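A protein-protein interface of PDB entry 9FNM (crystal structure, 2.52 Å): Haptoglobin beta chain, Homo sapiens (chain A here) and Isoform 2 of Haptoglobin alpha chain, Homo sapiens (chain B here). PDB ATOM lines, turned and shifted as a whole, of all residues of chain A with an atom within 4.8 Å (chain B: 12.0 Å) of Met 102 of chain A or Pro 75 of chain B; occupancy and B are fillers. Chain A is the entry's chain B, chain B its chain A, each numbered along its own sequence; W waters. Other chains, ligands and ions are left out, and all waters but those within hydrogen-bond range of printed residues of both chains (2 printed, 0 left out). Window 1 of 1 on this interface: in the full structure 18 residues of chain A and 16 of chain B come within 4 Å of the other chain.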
ATOM      1  N   SER A  11       8.135   5.728  12.816  1.00  0.00           N
ATOM      2  CA  SER A  11       7.523   6.678  13.735  1.00  0.00           C
ATOM      3  C   SER A  11       8.528   7.336  14.670  1.00  0.00           C
ATOM      4  O   SER A  11       8.123   8.071  15.576  1.00  0.00           O
ATOM      5  CB  SER A  11       6.434   5.983  14.556  1.00  0.00           C
ATOM      6  OG  SER A  11       6.966   4.874  15.255  1.00  0.00           O
ATOM      7  N   PRO A  13      11.674   9.321  13.724  1.00  0.00           N
ATOM      8  CA  PRO A  13      12.696   9.920  12.850  1.00  0.00           C
ATOM      9  C   PRO A  13      13.845  10.566  13.606  1.00  0.00           C
ATOM     10  O   PRO A  13      14.838  10.952  12.973  1.00  0.00           O
ATOM     11  CB  PRO A  13      11.904  10.958  12.050  1.00  0.00           C
ATOM     12  CG  PRO A  13      10.790  11.347  12.970  1.00  0.00           C
ATOM     13  CD  PRO A  13      10.420  10.098  13.722  1.00  0.00           C
ATOM     14  N   TRP A  14      13.746  10.699  14.927  1.00  0.00           N
ATOM     15  CA  TRP A  14      14.837  11.235  15.729  1.00  0.00           C
ATOM     16  C   TRP A  14      15.835  10.170  16.157  1.00  0.00           C
ATOM     17  O   TRP A  14      16.881  10.515  16.721  1.00  0.00           O
ATOM     18  CB  TRP A  14      14.273  11.939  16.966  1.00  0.00           C
ATOM     19  CG  TRP A  14      13.235  11.127  17.674  1.00  0.00           C
ATOM     20  CD1 TRP A  14      13.452  10.106  18.552  1.00  0.00           C
ATOM     21  CD2 TRP A  14      11.810  11.260  17.558  1.00  0.00           C
ATOM     22  NE1 TRP A  14      12.254   9.598  18.994  1.00  0.00           N
ATOM     23  CE2 TRP A  14      11.231  10.288  18.400  1.00  0.00           C
ATOM     24  CE3 TRP A  14      10.970  12.108  16.830  1.00  0.00           C
ATOM     25  CZ2 TRP A  14       9.852  10.142  18.531  1.00  0.00           C
ATOM     26  CZ3 TRP A  14       9.600  11.961  16.963  1.00  0.00           C
ATOM     27  CH2 TRP A  14       9.055  10.984  17.807  1.00  0.00           C
ATOM     28  N   LEU A  30      18.395  12.711  17.770  1.00  0.00           N
ATOM     29  CA  LEU A  30      18.431  14.001  17.092  1.00  0.00           C
ATOM     30  C   LEU A  30      17.511  14.986  17.811  1.00  0.00           C
ATOM     31  O   LEU A  30      16.296  14.774  17.887  1.00  0.00           O
ATOM     32  CB  LEU A  30      18.014  13.828  15.631  1.00  0.00           C
ATOM     33  CG  LEU A  30      18.383  14.917  14.619  1.00  0.00           C
ATOM     34  CD1 LEU A  30      19.898  15.017  14.449  1.00  0.00           C
ATOM     35  CD2 LEU A  30      17.698  14.664  13.274  1.00  0.00           C
ATOM     36  N   VAL A  97      15.783  17.497   6.864  1.00  0.00           N
ATOM     37  CA  VAL A  97      14.684  16.979   7.673  1.00  0.00           C
ATOM     38  C   VAL A  97      13.538  16.559   6.765  1.00  0.00           C
ATOM     39  O   VAL A  97      13.047  17.357   5.957  1.00  0.00           O
ATOM     40  CB  VAL A  97      14.217  18.017   8.706  1.00  0.00           C
ATOM     41  CG1 VAL A  97      12.982  17.511   9.440  1.00  0.00           C
ATOM     42  CG2 VAL A  97      15.340  18.307   9.686  1.00  0.00           C
ATOM     43  N   ASN A  98      13.102  15.313   6.908  1.00  0.00           N
ATOM     44  CA  ASN A  98      11.990  14.768   6.138  1.00  0.00           C
ATOM     45  C   ASN A  98      11.226  13.802   7.037  1.00  0.00           C
ATOM     46  O   ASN A  98      11.320  13.880   8.266  1.00  0.00           O
ATOM     47  CB  ASN A  98      12.511  14.123   4.843  1.00  0.00           C
ATOM     48  CG  ASN A  98      13.671  13.180   5.088  1.00  0.00           C
ATOM     49  OD1 ASN A  98      13.591  12.280   5.924  1.00  0.00           O
ATOM     50  ND2 ASN A  98      14.767  13.396   4.370  1.00  0.00           N
ATOM     51  N   ARG A 100      11.725  10.642   7.383  1.00  0.00           N
ATOM     52  CA  ARG A 100      12.618   9.653   7.970  1.00  0.00           C
ATOM     53  C   ARG A 100      13.647  10.249   8.917  1.00  0.00           C
ATOM     54  O   ARG A 100      14.218   9.509   9.726  1.00  0.00           O
ATOM     55  CB  ARG A 100      13.354   8.875   6.871  1.00  0.00           C
ATOM     56  CG  ARG A 100      12.541   7.756   6.250  1.00  0.00           C
ATOM     57  CD  ARG A 100      13.448   6.631   5.782  1.00  0.00           C
ATOM     58  NE  ARG A 100      12.758   5.347   5.760  1.00  0.00           N
ATOM     59  CZ  ARG A 100      12.304   4.757   4.662  1.00  0.00           C
ATOM     60  NH1 ARG A 100      12.473   5.298   3.467  1.00  0.00           N
ATOM     61  NH2 ARG A 100      11.665   3.596   4.767  1.00  0.00           N
ATOM     62  N   VAL A 101      13.904  11.555   8.838  1.00  0.00           N
ATOM     63  CA  VAL A 101      14.903  12.212   9.677  1.00  0.00           C
ATOM     64  C   VAL A 101      14.277  13.491  10.220  1.00  0.00           C
ATOM     65  O   VAL A 101      13.976  14.409   9.451  1.00  0.00           O
ATOM     66  CB  VAL A 101      16.200  12.527   8.913  1.00  0.00           C
ATOM     67  CG1 VAL A 101      17.195  13.252   9.814  1.00  0.00           C
ATOM     68  CG2 VAL A 101      16.808  11.251   8.341  1.00  0.00           C
ATOM     69  N   MET A 102      14.087  13.557  11.542  1.00  0.00           N
ATOM     70  CA  MET A 102      13.440  14.707  12.155  1.00  0.00           C
ATOM     71  C   MET A 102      13.788  14.754  13.635  1.00  0.00           C
ATOM     72  O   MET A 102      13.660  13.730  14.318  1.00  0.00           O
ATOM     73  CB  MET A 102      11.921  14.644  11.979  1.00  0.00           C
ATOM     74  CG  MET A 102      11.185  15.773  12.672  1.00  0.00           C
ATOM     75  SD  MET A 102       9.423  15.446  12.790  1.00  0.00           S
ATOM     76  CE  MET A 102       9.096  14.811  11.147  1.00  0.00           C
ATOM     77  N   PRO A 103      14.195  15.908  14.160  1.00  0.00           N
ATOM     78  CA  PRO A 103      14.541  15.985  15.584  1.00  0.00           C
ATOM     79  C   PRO A 103      13.310  15.931  16.470  1.00  0.00           C
ATOM     80  O   PRO A 103      12.207  16.307  16.071  1.00  0.00           O
ATOM     81  CB  PRO A 103      15.249  17.341  15.703  1.00  0.00           C
ATOM     82  CG  PRO A 103      14.702  18.141  14.575  1.00  0.00           C
ATOM     83  CD  PRO A 103      14.494  17.161  13.455  1.00  0.00           C
ATOM     84  N   ILE A 104      13.510  15.433  17.674  1.00  0.00           N
ATOM     85  CA  ILE A 104      12.488  15.434  18.712  1.00  0.00           C
ATOM     86  C   ILE A 104      12.606  16.736  19.492  1.00  0.00           C
ATOM     87  O   ILE A 104      13.672  17.359  19.543  1.00  0.00           O
ATOM     88  CB  ILE A 104      12.640  14.194  19.620  1.00  0.00           C
ATOM     89  CG1 ILE A 104      11.372  13.960  20.439  1.00  0.00           C
ATOM     90  CG2 ILE A 104      13.865  14.322  20.523  1.00  0.00           C
ATOM     91  CD1 ILE A 104      11.404  12.677  21.233  1.00  0.00           C
ATOM     92  N   TRP A 208       5.873  15.339  20.255  1.00  0.00           N
ATOM     93  CA  TRP A 208       6.679  14.311  20.895  1.00  0.00           C
ATOM     94  C   TRP A 208       7.916  14.938  21.522  1.00  0.00           C
ATOM     95  O   TRP A 208       8.623  15.717  20.874  1.00  0.00           O
ATOM     96  CB  TRP A 208       7.071  13.235  19.885  1.00  0.00           C
ATOM     97  CG  TRP A 208       5.884  12.471  19.401  1.00  0.00           C
ATOM     98  CD1 TRP A 208       4.909  12.921  18.563  1.00  0.00           C
ATOM     99  CD2 TRP A 208       5.531  11.127  19.744  1.00  0.00           C
ATOM    100  NE1 TRP A 208       3.973  11.939  18.355  1.00  0.00           N
ATOM    101  CE2 TRP A 208       4.332  10.827  19.068  1.00  0.00           C
ATOM    102  CE3 TRP A 208       6.115  10.147  20.552  1.00  0.00           C
ATOM    103  CZ2 TRP A 208       3.705   9.589  19.176  1.00  0.00           C
ATOM    104  CZ3 TRP A 208       5.493   8.917  20.657  1.00  0.00           C
ATOM    105  CH2 TRP A 208       4.299   8.649  19.970  1.00  0.00           C
ATOM    106  N   LYS B  35       9.121  24.972   2.949  1.00  0.00           N
ATOM    107  CA  LYS B  35       8.600  23.663   2.603  1.00  0.00           C
ATOM    108  C   LYS B  35       8.453  22.814   3.861  1.00  0.00           C
ATOM    109  O   LYS B  35       8.861  23.200   4.960  1.00  0.00           O
ATOM    110  CB  LYS B  35       9.526  22.958   1.613  1.00  0.00           C
ATOM    111  CG  LYS B  35      10.215  23.879   0.624  1.00  0.00           C
ATOM    112  CD  LYS B  35      11.137  23.098  -0.302  1.00  0.00           C
ATOM    113  CE  LYS B  35      11.821  24.010  -1.305  1.00  0.00           C
ATOM    114  NZ  LYS B  35      12.621  23.239  -2.298  1.00  0.00           N
ATOM    115  N   ASN B  36       7.855  21.640   3.692  1.00  0.00           N
ATOM    116  CA  ASN B  36       7.977  20.614   4.715  1.00  0.00           C
ATOM    117  C   ASN B  36       9.430  20.154   4.782  1.00  0.00           C
ATOM    118  O   ASN B  36      10.124  20.077   3.763  1.00  0.00           O
ATOM    119  CB  ASN B  36       7.060  19.434   4.399  1.00  0.00           C
ATOM    120  CG  ASN B  36       5.952  19.798   3.432  1.00  0.00           C
ATOM    121  OD1 ASN B  36       5.358  20.873   3.521  1.00  0.00           O
ATOM    122  ND2 ASN B  36       5.672  18.902   2.493  1.00  0.00           N
ATOM    123  N   TYR B  37       9.905  19.859   5.989  1.00  0.00           N
ATOM    124  CA  TYR B  37       9.118  19.905   7.215  1.00  0.00           C
ATOM    125  C   TYR B  37       9.626  21.048   8.082  1.00  0.00           C
ATOM    126  O   TYR B  37      10.169  20.820   9.162  1.00  0.00           O
ATOM    127  CB  TYR B  37       9.219  18.577   7.979  1.00  0.00           C
ATOM    128  CG  TYR B  37       8.680  17.361   7.245  1.00  0.00           C
ATOM    129  CD1 TYR B  37       9.126  17.031   5.968  1.00  0.00           C
ATOM    130  CD2 TYR B  37       7.746  16.529   7.843  1.00  0.00           C
ATOM    131  CE1 TYR B  37       8.640  15.932   5.300  1.00  0.00           C
ATOM    132  CE2 TYR B  37       7.258  15.418   7.185  1.00  0.00           C
ATOM    133  CZ  TYR B  37       7.709  15.125   5.913  1.00  0.00           C
ATOM    134  OH  TYR B  37       7.229  14.023   5.246  1.00  0.00           O
ATOM    135  N   TYR B  38       9.451  22.279   7.607  1.00  0.00           N
ATOM    136  CA  TYR B  38      10.107  23.443   8.187  1.00  0.00           C
ATOM    137  C   TYR B  38       9.087  24.517   8.541  1.00  0.00           C
ATOM    138  O   TYR B  38       7.924  24.467   8.133  1.00  0.00           O
ATOM    139  CB  TYR B  38      11.163  24.011   7.227  1.00  0.00           C
ATOM    140  CG  TYR B  38      12.349  23.102   7.025  1.00  0.00           C
ATOM    141  CD1 TYR B  38      12.272  22.003   6.178  1.00  0.00           C
ATOM    142  CD2 TYR B  38      13.548  23.339   7.683  1.00  0.00           C
ATOM    143  CE1 TYR B  38      13.358  21.164   5.998  1.00  0.00           C
ATOM    144  CE2 TYR B  38      14.638  22.507   7.506  1.00  0.00           C
ATOM    145  CZ  TYR B  38      14.537  21.423   6.664  1.00  0.00           C
ATOM    146  OH  TYR B  38      15.624  20.599   6.488  1.00  0.00           O
ATOM    147  N   LYS B  39       9.549  25.500   9.315  1.00  0.00           N
ATOM    148  CA  LYS B  39       8.731  26.630   9.727  1.00  0.00           C
ATOM    149  C   LYS B  39       9.494  27.924   9.486  1.00  0.00           C
ATOM    150  O   LYS B  39      10.727  27.953   9.501  1.00  0.00           O
ATOM    151  CB  LYS B  39       8.325  26.527  11.206  1.00  0.00           C
ATOM    152  CG  LYS B  39       9.490  26.619  12.178  1.00  0.00           C
ATOM    153  CD  LYS B  39       9.006  26.796  13.610  1.00  0.00           C
ATOM    154  CE  LYS B  39       8.188  25.605  14.070  1.00  0.00           C
ATOM    155  NZ  LYS B  39       7.785  25.736  15.496  1.00  0.00           N
ATOM    156  N   GLU B  69      13.383  26.976   9.698  1.00  0.00           N
ATOM    157  CA  GLU B  69      13.839  26.107  10.771  1.00  0.00           C
ATOM    158  C   GLU B  69      13.043  24.809  10.752  1.00  0.00           C
ATOM    159  O   GLU B  69      11.848  24.808  10.444  1.00  0.00           O
ATOM    160  CB  GLU B  69      13.688  26.802  12.125  1.00  0.00           C
ATOM    161  CG  GLU B  69      14.307  26.059  13.295  1.00  0.00           C
ATOM    162  CD  GLU B  69      13.932  26.677  14.627  1.00  0.00           C
ATOM    163  OE1 GLU B  69      13.152  27.654  14.629  1.00  0.00           O
ATOM    164  OE2 GLU B  69      14.414  26.188  15.669  1.00  0.00           O
ATOM    165  N   ALA B  70      13.713  23.709  11.079  1.00  0.00           N
ATOM    166  CA  ALA B  70      13.063  22.408  11.067  1.00  0.00           C
ATOM    167  C   ALA B  70      12.065  22.290  12.211  1.00  0.00           C
ATOM    168  O   ALA B  70      12.269  22.822  13.306  1.00  0.00           O
ATOM    169  CB  ALA B  70      14.098  21.291  11.163  1.00  0.00           C
ATOM    170  N   VAL B  71      10.974  21.584  11.944  1.00  0.00           N
ATOM    171  CA  VAL B  71       9.961  21.332  12.962  1.00  0.00           C
ATOM    172  C   VAL B  71      10.358  20.095  13.753  1.00  0.00           C
ATOM    173  O   VAL B  71      10.739  19.070  13.175  1.00  0.00           O
ATOM    174  CB  VAL B  71       8.576  21.161  12.320  1.00  0.00           C
ATOM    175  CG1 VAL B  71       7.516  20.987  13.385  1.00  0.00           C
ATOM    176  CG2 VAL B  71       8.257  22.358  11.444  1.00  0.00           C
ATOM    177  N   CYS B  72      10.273  20.183  15.074  1.00  0.00           N
ATOM    178  CA  CYS B  72      10.616  19.063  15.933  1.00  0.00           C
ATOM    179  C   CYS B  72       9.354  18.329  16.369  1.00  0.00           C
ATOM    180  O   CYS B  72       8.277  18.920  16.481  1.00  0.00           O
ATOM    181  CB  CYS B  72      11.408  19.529  17.162  1.00  0.00           C
ATOM    182  SG  CYS B  72      10.516  20.616  18.317  1.00  0.00           S
ATOM    183  N   GLY B  73       9.503  17.030  16.610  1.00  0.00           N
ATOM    184  CA  GLY B  73       8.459  16.244  17.254  1.00  0.00           C
ATOM    185  C   GLY B  73       7.108  16.239  16.573  1.00  0.00           C
ATOM    186  O   GLY B  73       6.075  16.259  17.254  1.00  0.00           O
ATOM    187  N   LYS B  74       7.085  16.210  15.244  1.00  0.00           N
ATOM    188  CA  LYS B  74       5.845  16.093  14.475  1.00  0.00           C
ATOM    189  C   LYS B  74       6.003  14.964  13.467  1.00  0.00           C
ATOM    190  O   LYS B  74       6.073  15.201  12.255  1.00  0.00           O
ATOM    191  CB  LYS B  74       5.497  17.408  13.775  1.00  0.00           C
ATOM    192  CG  LYS B  74       5.247  18.579  14.711  1.00  0.00           C
ATOM    193  CD  LYS B  74       3.925  18.445  15.446  1.00  0.00           C
ATOM    194  CE  LYS B  74       3.697  19.641  16.359  1.00  0.00           C
ATOM    195  NZ  LYS B  74       2.411  19.549  17.102  1.00  0.00           N
ATOM    196  N   PRO B  75       6.064  13.718  13.936  1.00  0.00           N
ATOM    197  CA  PRO B  75       6.317  12.600  13.020  1.00  0.00           C
ATOM    198  C   PRO B  75       5.196  12.448  12.004  1.00  0.00           C
ATOM    199  O   PRO B  75       4.017  12.632  12.317  1.00  0.00           O
ATOM    200  CB  PRO B  75       6.402  11.388  13.955  1.00  0.00           C
ATOM    201  CG  PRO B  75       5.625  11.790  15.166  1.00  0.00           C
ATOM    202  CD  PRO B  75       5.852  13.265  15.322  1.00  0.00           C
ATOM    203  N   LYS B  76       5.581  12.122  10.767  1.00  0.00           N
ATOM    204  CA  LYS B  76       4.593  11.961   9.707  1.00  0.00           C
ATOM    205  C   LYS B  76       3.645  10.808  10.004  1.00  0.00           C
ATOM    206  O   LYS B  76       2.434  10.916   9.784  1.00  0.00           O
ATOM    207  CB  LYS B  76       5.295  11.750   8.364  1.00  0.00           C
ATOM    208  CG  LYS B  76       4.341  11.564   7.197  1.00  0.00           C
ATOM    209  CD  LYS B  76       3.386  12.739   7.086  1.00  0.00           C
ATOM    210  CE  LYS B  76       4.141  14.031   6.819  1.00  0.00           C
ATOM    211  NZ  LYS B  76       3.551  15.189   7.548  1.00  0.00           N
ATOM    212  N   ASN B  77       4.179   9.694  10.506  1.00  0.00           N
ATOM    213  CA  ASN B  77       3.397   8.513  10.858  1.00  0.00           C
ATOM    214  C   ASN B  77       3.677   8.198  12.323  1.00  0.00           C
ATOM    215  O   ASN B  77       4.528   7.353  12.630  1.00  0.00           O
ATOM    216  CB  ASN B  77       3.746   7.321   9.967  1.00  0.00           C
ATOM    217  CG  ASN B  77       3.772   7.679   8.494  1.00  0.00           C
ATOM    218  OD1 ASN B  77       4.829   7.981   7.935  1.00  0.00           O
ATOM    219  ND2 ASN B  77       2.610   7.636   7.852  1.00  0.00           N
ATOM    220  N   PRO B  78       2.981   8.856  13.251  1.00  0.00           N
ATOM    221  CA  PRO B  78       3.269   8.645  14.674  1.00  0.00           C
ATOM    222  C   PRO B  78       2.943   7.225  15.114  1.00  0.00           C
ATOM    223  O   PRO B  78       2.159   6.511  14.486  1.00  0.00           O
ATOM    224  CB  PRO B  78       2.367   9.668  15.375  1.00  0.00           C
ATOM    225  CG  PRO B  78       1.260   9.920  14.400  1.00  0.00           C
ATOM    226  CD  PRO B  78       1.889   9.821  13.041  1.00  0.00           C
ATOM    227  N   ALA B  79       3.572   6.816  16.213  1.00  0.00           N
ATOM    228  CA  ALA B  79       3.359   5.480  16.741  1.00  0.00           C
ATOM    229  C   ALA B  79       1.923   5.322  17.235  1.00  0.00           C
ATOM    230  O   ALA B  79       1.223   6.297  17.524  1.00  0.00           O
ATOM    231  CB  ALA B  79       4.347   5.182  17.871  1.00  0.00           C
ATOM    232  N   ASN B  80       1.490   4.068  17.323  1.00  0.00           N
ATOM    233  CA  ASN B  80       0.130   3.779  17.750  1.00  0.00           C
ATOM    234  C   ASN B  80      -0.091   4.280  19.175  1.00  0.00           C
ATOM    235  O   ASN B  80       0.792   4.132  20.031  1.00  0.00           O
ATOM    236  CB  ASN B  80      -0.150   2.279  17.658  1.00  0.00           C
ATOM    237  CG  ASN B  80       1.086   1.439  17.907  1.00  0.00           C
ATOM    238  OD1 ASN B  80       1.961   1.816  18.686  1.00  0.00           O
ATOM    239  ND2 ASN B  80       1.168   0.295  17.235  1.00  0.00           N
ATOM    240  N   PRO B  81      -1.243   4.886  19.460  1.00  0.00           N
ATOM    241  CA  PRO B  81      -1.449   5.530  20.764  1.00  0.00           C
ATOM    242  C   PRO B  81      -1.392   4.536  21.915  1.00  0.00           C
ATOM    243  O   PRO B  81      -1.424   3.316  21.743  1.00  0.00           O
ATOM    244  CB  PRO B  81      -2.842   6.155  20.632  1.00  0.00           C
ATOM    245  CG  PRO B  81      -3.037   6.328  19.159  1.00  0.00           C
ATOM    246  CD  PRO B  81      -2.356   5.150  18.533  1.00  0.00           C
HETATM  247  O   HOH W   1       6.086   8.184  16.925  1.00  0.00           O
HETATM  248  O   HOH W   2      11.789  17.881   3.419  1.00  0.00           O
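Printed residues of chain A that touch a printed residue of chain B: Ser 11, Val 97, Asn 98, Met 102, Pro 103, Ile 104 and Trp 208. Hydrophobic or aromatic side chains of chain A within 4 Å of the printed part of chain B: Val 97, Met 102 and Trp 208. Among the printed residues, 17 pairs touch across the chains.
Of chain B, only Asn 77, Pro 78 and Ala 79 come within 4 Å of Ser 11 of chain A. No residue of chain B comes within 4 Å of Pro 13 of chain A. No residue of chain B comes within 4 Å of Trp 14 of chain A. Asn 98 of chain A touches just one residue of chain B: Tyr 37 (3.6 Å). Pro 103 of chain A touches just these residues of chain B: Cys 72 (3.2 Å) and Gly 73 (2.9 Å). Of chain B, only Gly 73 (3.1 Å) and Pro 75 (3.4 Å) come within 4 Å of Trp 208 of chain A. Of the printed residues of chain A, Tyr 37 of chain B touches Val 97, Asn 98 and Met 102. Of the printed residues of chain A, Cys 72 of chain B touches Pro 103 and Ile 104. Of chain A, only Met 102 and Trp 208 come within 4 Å of Pro 75 of chain B.
Water W1 bridges O of Ser 11 of chain A and N of Ala 79 of chain B. Water W2 bridges O of Asn 36 of chain B (2.8 Å) and O of Val 97 of chain A (2.9 Å).
The backbone carbonyl oxygen (O) of Gly 73 of chain B lies within hydrogen-bond range of the backbone NH (N) of Trp 208 of chain A (3.1 Å). The backbone NH of Val 97 of chain A lies within hydrogen-bond range of the side-chain hydroxyl of Tyr 38 of chain B (3.1 Å). The backbone NH (N) of Gly 73 of chain B sits at hydrogen-bond distance from the backbone carbonyl oxygen (O) of Pro 103 of chain A, 2.9 Å away. The backbone NH (N) of Lys 74 of chain B is in hydrogen-bond range of the side-chain sulfur (SD) of Met 102 of chain A (3.5 Å).
The backbone NH of Val 71 of chain B sits at hydrogen-bond distance from the backbone carbonyl oxygen of Tyr 37 of chain B (3.0 Å). O of Leu 30 of chain A is in hydrogen-bond range of N of Ile 104 of chain A (2.9 Å). The backbone NH of Trp 14 of chain A is in hydrogen-bond range of the backbone carbonyl oxygen of Met 102 of chain A (3.1 Å). The backbone NH (N) of Met 102 of chain A is in hydrogen-bond range of the backbone carbonyl oxygen (O) of Pro 13 of chain A. The side-chain amide oxygen (OD1) of Asn 98 of chain A is in hydrogen-bond range of the backbone NH (N) of Arg 100 of chain A (2.9 Å). The backbone NH (N) of Val 101 of chain A sits at hydrogen-bond distance from the side-chain amide oxygen (OD1) of Asn 98 of chain A, 3.0 Å away.
Among the printed residues, merely in contact across the chains: Ser 11 of chain A with Asn 77 of chain B (3.0 Å), Ser 11 of chain A with Pro 78 of chain B (3.7 Å), Ser 11 of chain A with Ala 79 of chain B (3.4 Å), Val 97 of chain A with Tyr 37 of chain B (3.9 Å), Val 97 of chain A with Ala 70 of chain B (3.6 Å), Asn 98 of chain A with Tyr 37 of chain B (3.6 Å), Met 102 of chain A with Tyr 37 of chain B (3.96 Å), Met 102 of chain A with Val 71 of chain B (3.4 Å), Met 102 of chain A with Pro 75 of chain B (3.9 Å), Pro 103 of chain A with Cys 72 of chain B (3.2 Å), Ile 104 of chain A with Cys 72 of chain B (3.8 Å), Ile 104 of chain A with Gly 73 of chain B (3.98 Å) and Trp 208 of chain A with Pro 75 of chain B (3.4 Å).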
